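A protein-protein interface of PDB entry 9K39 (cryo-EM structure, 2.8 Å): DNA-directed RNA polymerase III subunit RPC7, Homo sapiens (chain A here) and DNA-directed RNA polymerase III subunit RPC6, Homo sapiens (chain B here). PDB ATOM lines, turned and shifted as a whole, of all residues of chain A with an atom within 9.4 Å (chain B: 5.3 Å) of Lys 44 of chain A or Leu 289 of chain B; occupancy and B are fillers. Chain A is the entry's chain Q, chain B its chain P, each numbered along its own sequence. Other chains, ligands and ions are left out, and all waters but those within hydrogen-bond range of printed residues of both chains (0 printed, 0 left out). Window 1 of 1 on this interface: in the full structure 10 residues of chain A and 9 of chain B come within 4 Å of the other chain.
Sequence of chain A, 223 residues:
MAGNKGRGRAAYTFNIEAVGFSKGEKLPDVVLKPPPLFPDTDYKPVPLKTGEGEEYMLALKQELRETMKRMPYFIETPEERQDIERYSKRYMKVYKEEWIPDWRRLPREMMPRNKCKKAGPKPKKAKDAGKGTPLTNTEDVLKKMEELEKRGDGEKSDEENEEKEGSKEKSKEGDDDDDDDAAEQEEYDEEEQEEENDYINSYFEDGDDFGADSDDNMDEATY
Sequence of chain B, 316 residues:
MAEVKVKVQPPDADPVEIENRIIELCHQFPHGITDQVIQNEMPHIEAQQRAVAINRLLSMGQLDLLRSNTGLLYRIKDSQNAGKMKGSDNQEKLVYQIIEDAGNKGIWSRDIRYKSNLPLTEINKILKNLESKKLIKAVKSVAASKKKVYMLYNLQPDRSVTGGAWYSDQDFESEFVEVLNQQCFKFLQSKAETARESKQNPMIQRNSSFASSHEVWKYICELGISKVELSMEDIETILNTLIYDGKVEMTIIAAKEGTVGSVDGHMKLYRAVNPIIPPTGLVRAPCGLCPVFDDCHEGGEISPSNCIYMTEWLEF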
ATOM      1  N   PRO A  39      15.737   1.624   4.248  1.00  0.00           N
ATOM      2  CA  PRO A  39      15.803   0.268   4.808  1.00  0.00           C
ATOM      3  C   PRO A  39      14.469  -0.453   4.682  1.00  0.00           C
ATOM      4  O   PRO A  39      13.400   0.146   4.814  1.00  0.00           O
ATOM      5  CB  PRO A  39      16.178   0.510   6.274  1.00  0.00           C
ATOM      6  CG  PRO A  39      15.692   1.893   6.560  1.00  0.00           C
ATOM      7  CD  PRO A  39      15.885   2.659   5.284  1.00  0.00           C
ATOM      8  N   ASP A  40      14.543  -1.756   4.424  1.00  0.00           N
ATOM      9  CA  ASP A  40      13.339  -2.550   4.232  1.00  0.00           C
ATOM     10  C   ASP A  40      12.634  -2.799   5.562  1.00  0.00           C
ATOM     11  O   ASP A  40      13.262  -2.877   6.622  1.00  0.00           O
ATOM     12  CB  ASP A  40      13.680  -3.882   3.564  1.00  0.00           C
ATOM     13  CG  ASP A  40      14.803  -4.619   4.267  1.00  0.00           C
ATOM     14  OD1 ASP A  40      15.447  -4.023   5.156  1.00  0.00           O
ATOM     15  OD2 ASP A  40      15.043  -5.798   3.933  1.00  0.00           O
ATOM     16  N   THR A  41      11.311  -2.925   5.496  1.00  0.00           N
ATOM     17  CA  THR A  41      10.481  -3.188   6.660  1.00  0.00           C
ATOM     18  C   THR A  41       9.596  -4.394   6.389  1.00  0.00           C
ATOM     19  O   THR A  41       9.039  -4.533   5.295  1.00  0.00           O
ATOM     20  CB  THR A  41       9.611  -1.976   7.023  1.00  0.00           C
ATOM     21  OG1 THR A  41       8.799  -1.616   5.899  1.00  0.00           O
ATOM     22  CG2 THR A  41      10.480  -0.793   7.418  1.00  0.00           C
ATOM     23  N   ASP A  42       9.467  -5.264   7.390  1.00  0.00           N
ATOM     24  CA  ASP A  42       8.646  -6.460   7.265  1.00  0.00           C
ATOM     25  C   ASP A  42       7.160  -6.185   7.448  1.00  0.00           C
ATOM     26  O   ASP A  42       6.345  -7.079   7.188  1.00  0.00           O
ATOM     27  CB  ASP A  42       9.103  -7.517   8.275  1.00  0.00           C
ATOM     28  CG  ASP A  42       9.245  -6.956   9.675  1.00  0.00           C
ATOM     29  OD1 ASP A  42       9.178  -5.719   9.829  1.00  0.00           O
ATOM     30  OD2 ASP A  42       9.427  -7.753  10.620  1.00  0.00           O
ATOM     31  N   TYR A  43       6.784  -4.987   7.883  1.00  0.00           N
ATOM     32  CA  TYR A  43       5.388  -4.606   8.047  1.00  0.00           C
ATOM     33  C   TYR A  43       4.983  -3.680   6.907  1.00  0.00           C
ATOM     34  O   TYR A  43       5.666  -2.689   6.635  1.00  0.00           O
ATOM     35  CB  TYR A  43       5.157  -3.918   9.396  1.00  0.00           C
ATOM     36  CG  TYR A  43       5.419  -4.809  10.588  1.00  0.00           C
ATOM     37  CD1 TYR A  43       4.474  -5.737  11.008  1.00  0.00           C
ATOM     38  CD2 TYR A  43       6.608  -4.717  11.298  1.00  0.00           C
ATOM     39  CE1 TYR A  43       4.711  -6.553  12.098  1.00  0.00           C
ATOM     40  CE2 TYR A  43       6.854  -5.529  12.390  1.00  0.00           C
ATOM     41  CZ  TYR A  43       5.901  -6.444  12.788  1.00  0.00           C
ATOM     42  OH  TYR A  43       6.142  -7.253  13.873  1.00  0.00           O
ATOM     43  N   LYS A  44       3.880  -4.009   6.249  1.00  0.00           N
ATOM     44  CA  LYS A  44       3.374  -3.247   5.121  1.00  0.00           C
ATOM     45  C   LYS A  44       2.132  -2.461   5.519  1.00  0.00           C
ATOM     46  O   LYS A  44       1.419  -2.837   6.456  1.00  0.00           O
ATOM     47  CB  LYS A  44       3.043  -4.178   3.946  1.00  0.00           C
ATOM     48  CG  LYS A  44       4.198  -5.072   3.519  1.00  0.00           C
ATOM     49  CD  LYS A  44       5.430  -4.259   3.152  1.00  0.00           C
ATOM     50  CE  LYS A  44       5.174  -3.378   1.938  1.00  0.00           C
ATOM     51  NZ  LYS A  44       6.369  -2.561   1.585  1.00  0.00           N
ATOM     52  N   PRO A  45       1.852  -1.350   4.838  1.00  0.00           N
ATOM     53  CA  PRO A  45       0.660  -0.563   5.173  1.00  0.00           C
ATOM     54  C   PRO A  45      -0.617  -1.366   4.974  1.00  0.00           C
ATOM     55  O   PRO A  45      -0.732  -2.169   4.043  1.00  0.00           O
ATOM     56  CB  PRO A  45       0.737   0.625   4.209  1.00  0.00           C
ATOM     57  CG  PRO A  45       2.182   0.737   3.861  1.00  0.00           C
ATOM     58  CD  PRO A  45       2.692  -0.673   3.835  1.00  0.00           C
ATOM     59  N   VAL A  46      -1.579  -1.144   5.868  1.00  0.00           N
ATOM     60  CA  VAL A  46      -2.872  -1.826   5.767  1.00  0.00           C
ATOM     61  C   VAL A  46      -3.584  -1.358   4.505  1.00  0.00           C
ATOM     62  O   VAL A  46      -3.553  -0.151   4.191  1.00  0.00           O
ATOM     63  CB  VAL A  46      -3.722  -1.549   7.019  1.00  0.00           C
ATOM     64  CG1 VAL A  46      -5.085  -2.216   6.914  1.00  0.00           C
ATOM     65  CG2 VAL A  46      -2.990  -2.017   8.269  1.00  0.00           C
ATOM     66  N   PRO A  47      -4.211  -2.246   3.733  1.00  0.00           N
ATOM     67  CA  PRO A  47      -4.961  -1.796   2.555  1.00  0.00           C
ATOM     68  C   PRO A  47      -6.081  -0.841   2.937  1.00  0.00           C
ATOM     69  O   PRO A  47      -6.671  -0.933   4.017  1.00  0.00           O
ATOM     70  CB  PRO A  47      -5.509  -3.099   1.958  1.00  0.00           C
ATOM     71  CG  PRO A  47      -5.416  -4.106   3.066  1.00  0.00           C
ATOM     72  CD  PRO A  47      -4.209  -3.714   3.855  1.00  0.00           C
ATOM     73  N   LEU B 282      -4.101   6.346   9.156  1.00  0.00           N
ATOM     74  CA  LEU B 282      -2.682   6.681   9.079  1.00  0.00           C
ATOM     75  C   LEU B 282      -1.851   5.478   8.654  1.00  0.00           C
ATOM     76  O   LEU B 282      -0.940   5.603   7.827  1.00  0.00           O
ATOM     77  CB  LEU B 282      -2.192   7.216  10.424  1.00  0.00           C
ATOM     78  CG  LEU B 282      -0.680   7.444  10.519  1.00  0.00           C
ATOM     79  CD1 LEU B 282      -0.237   8.553   9.575  1.00  0.00           C
ATOM     80  CD2 LEU B 282      -0.265   7.750  11.949  1.00  0.00           C
ATOM     81  N   VAL B 283      -2.152   4.300   9.207  1.00  0.00           N
ATOM     82  CA  VAL B 283      -1.390   3.100   8.883  1.00  0.00           C
ATOM     83  C   VAL B 283      -1.656   2.600   7.474  1.00  0.00           C
ATOM     84  O   VAL B 283      -0.908   1.751   6.976  1.00  0.00           O
ATOM     85  CB  VAL B 283      -1.693   1.980   9.898  1.00  0.00           C
ATOM     86  CG1 VAL B 283      -1.595   2.515  11.315  1.00  0.00           C
ATOM     87  CG2 VAL B 283      -3.065   1.380   9.642  1.00  0.00           C
ATOM     88  N   ALA B 285      -1.321   4.446   4.896  1.00  0.00           N
ATOM     89  CA  ALA B 285      -0.419   5.203   4.049  1.00  0.00           C
ATOM     90  C   ALA B 285       1.026   4.827   4.350  1.00  0.00           C
ATOM     91  O   ALA B 285       1.370   4.570   5.509  1.00  0.00           O
ATOM     92  CB  ALA B 285      -0.602   6.712   4.249  1.00  0.00           C
ATOM     93  N   PRO B 286       1.890   4.773   3.332  1.00  0.00           N
ATOM     94  CA  PRO B 286       3.297   4.415   3.587  1.00  0.00           C
ATOM     95  C   PRO B 286       4.017   5.398   4.492  1.00  0.00           C
ATOM     96  O   PRO B 286       4.998   5.020   5.146  1.00  0.00           O
ATOM     97  CB  PRO B 286       3.910   4.388   2.181  1.00  0.00           C
ATOM     98  CG  PRO B 286       2.752   4.180   1.259  1.00  0.00           C
ATOM     99  CD  PRO B 286       1.604   4.905   1.894  1.00  0.00           C
ATOM    100  N   CYS B 287       3.563   6.652   4.549  1.00  0.00           N
ATOM    101  CA  CYS B 287       4.233   7.648   5.379  1.00  0.00           C
ATOM    102  C   CYS B 287       4.080   7.343   6.863  1.00  0.00           C
ATOM    103  O   CYS B 287       4.975   7.659   7.656  1.00  0.00           O
ATOM    104  CB  CYS B 287       3.683   9.041   5.070  1.00  0.00           C
ATOM    105  SG  CYS B 287       3.397   9.364   3.313  1.00  0.00           S
ATOM    106  N   GLY B 288       2.961   6.731   7.257  1.00  0.00           N
ATOM    107  CA  GLY B 288       2.726   6.439   8.660  1.00  0.00           C
ATOM    108  C   GLY B 288       3.534   5.275   9.196  1.00  0.00           C
ATOM    109  O   GLY B 288       3.757   5.197  10.409  1.00  0.00           O
ATOM    110  N   LEU B 289       3.974   4.373   8.322  1.00  0.00           N
ATOM    111  CA  LEU B 289       4.763   3.215   8.719  1.00  0.00           C
ATOM    112  C   LEU B 289       6.215   3.320   8.271  1.00  0.00           C
ATOM    113  O   LEU B 289       6.938   2.318   8.291  1.00  0.00           O
ATOM    114  CB  LEU B 289       4.134   1.934   8.167  1.00  0.00           C
ATOM    115  CG  LEU B 289       2.646   1.728   8.462  1.00  0.00           C
ATOM    116  CD1 LEU B 289       2.165   0.396   7.909  1.00  0.00           C
ATOM    117  CD2 LEU B 289       2.370   1.823   9.954  1.00  0.00           C
ATOM    118  N   CYS B 290       6.655   4.505   7.866  1.00  0.00           N
ATOM    119  CA  CYS B 290       8.017   4.669   7.378  1.00  0.00           C
ATOM    120  C   CYS B 290       8.999   4.695   8.545  1.00  0.00           C
ATOM    121  O   CYS B 290       8.758   5.388   9.540  1.00  0.00           O
ATOM    122  CB  CYS B 290       8.135   5.955   6.567  1.00  0.00           C
ATOM    123  SG  CYS B 290       9.802   6.279   5.958  1.00  0.00           S
ATOM    124  N   PRO B 291      10.114   3.959   8.464  1.00  0.00           N
ATOM    125  CA  PRO B 291      11.113   4.020   9.541  1.00  0.00           C
ATOM    126  C   PRO B 291      12.074   5.189   9.425  1.00  0.00           C
ATOM    127  O   PRO B 291      12.747   5.511  10.414  1.00  0.00           O
ATOM    128  CB  PRO B 291      11.853   2.684   9.402  1.00  0.00           C
ATOM    129  CG  PRO B 291      11.771   2.387   7.938  1.00  0.00           C
ATOM    130  CD  PRO B 291      10.445   2.935   7.457  1.00  0.00           C
ATOM    131  N   GLU B 312       6.155   1.256  -4.528  1.00  0.00           N
ATOM    132  CA  GLU B 312       5.725  -0.132  -4.399  1.00  0.00           C
ATOM    133  C   GLU B 312       4.273  -0.221  -3.942  1.00  0.00           C
ATOM    134  O   GLU B 312       3.550  -1.147  -4.323  1.00  0.00           O
ATOM    135  CB  GLU B 312       6.641  -0.880  -3.429  1.00  0.00           C
ATOM    136  CG  GLU B 312       8.095  -0.934  -3.867  1.00  0.00           C
ATOM    137  CD  GLU B 312       8.981  -1.629  -2.851  1.00  0.00           C
ATOM    138  OE1 GLU B 312       8.454  -2.072  -1.807  1.00  0.00           O
ATOM    139  OE2 GLU B 312      10.199  -1.734  -3.097  1.00  0.00           O
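Pro 291 of chain B touches Thr 41 of chain A (CG to CG2, 3.5 Å).
Lys 44 of chain A touches Leu 289 of chain B (O to CD1, 3.6 Å).
Pro 45 of chain A touches Val 283 of chain B.
CA of Pro 286 of chain B touches CG of Pro 45 of chain A (3.9 Å).
Pro 45 of chain A touches Leu 289 of chain B (CA to CD1, 3.3 Å).
Of the printed residues of chain B, Lys 44 of chain A touches Leu 289 (3.6 Å).
No residue of chain A comes within 4 Å of Gly 288 of chain B.
Printed residues of chain B within 4 Å of Val 46 of chain A: Val 283 (3.2 Å).
Of the printed residues of chain B, Pro 45 of chain A touches Val 283 (3.3 Å), Pro 286 (3.9 Å) and Leu 289 (3.3 Å).
The nearest residue of chain A that does not touch Leu 289 of chain B is Val 46 of chain A (4.5 Å).
Of the 9 printed residues of chain A, 4 touch a printed residue of chain B.
Hydrophobic or aromatic side chains of chain A that line the printed part of chain B: Pro 45 and Val 46.
Printed residues of chain B that touch a printed residue of chain A: Val 283, Pro 286, Leu 289 and Pro 291.
Hydrophobic or aromatic side chains of chain B within 4 Å of the printed part of chain A: Val 283, Leu 289 and Pro 291.
Among the printed residues, 6 pairs touch across the chains.
Among the printed residues, no Asp or Glu carboxylate lies within 4 Å of a Lys or Arg side-chain nitrogen of the other chain.
The backbone carbonyl oxygen of Tyr 43 of chain A is in hydrogen-bond range of the side-chain hydroxyl of Thr 41 of chain A (3.4 Å).
O of Val 283 of chain B is in hydrogen-bond range of N of Val 46 of chain A (3.2 Å).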
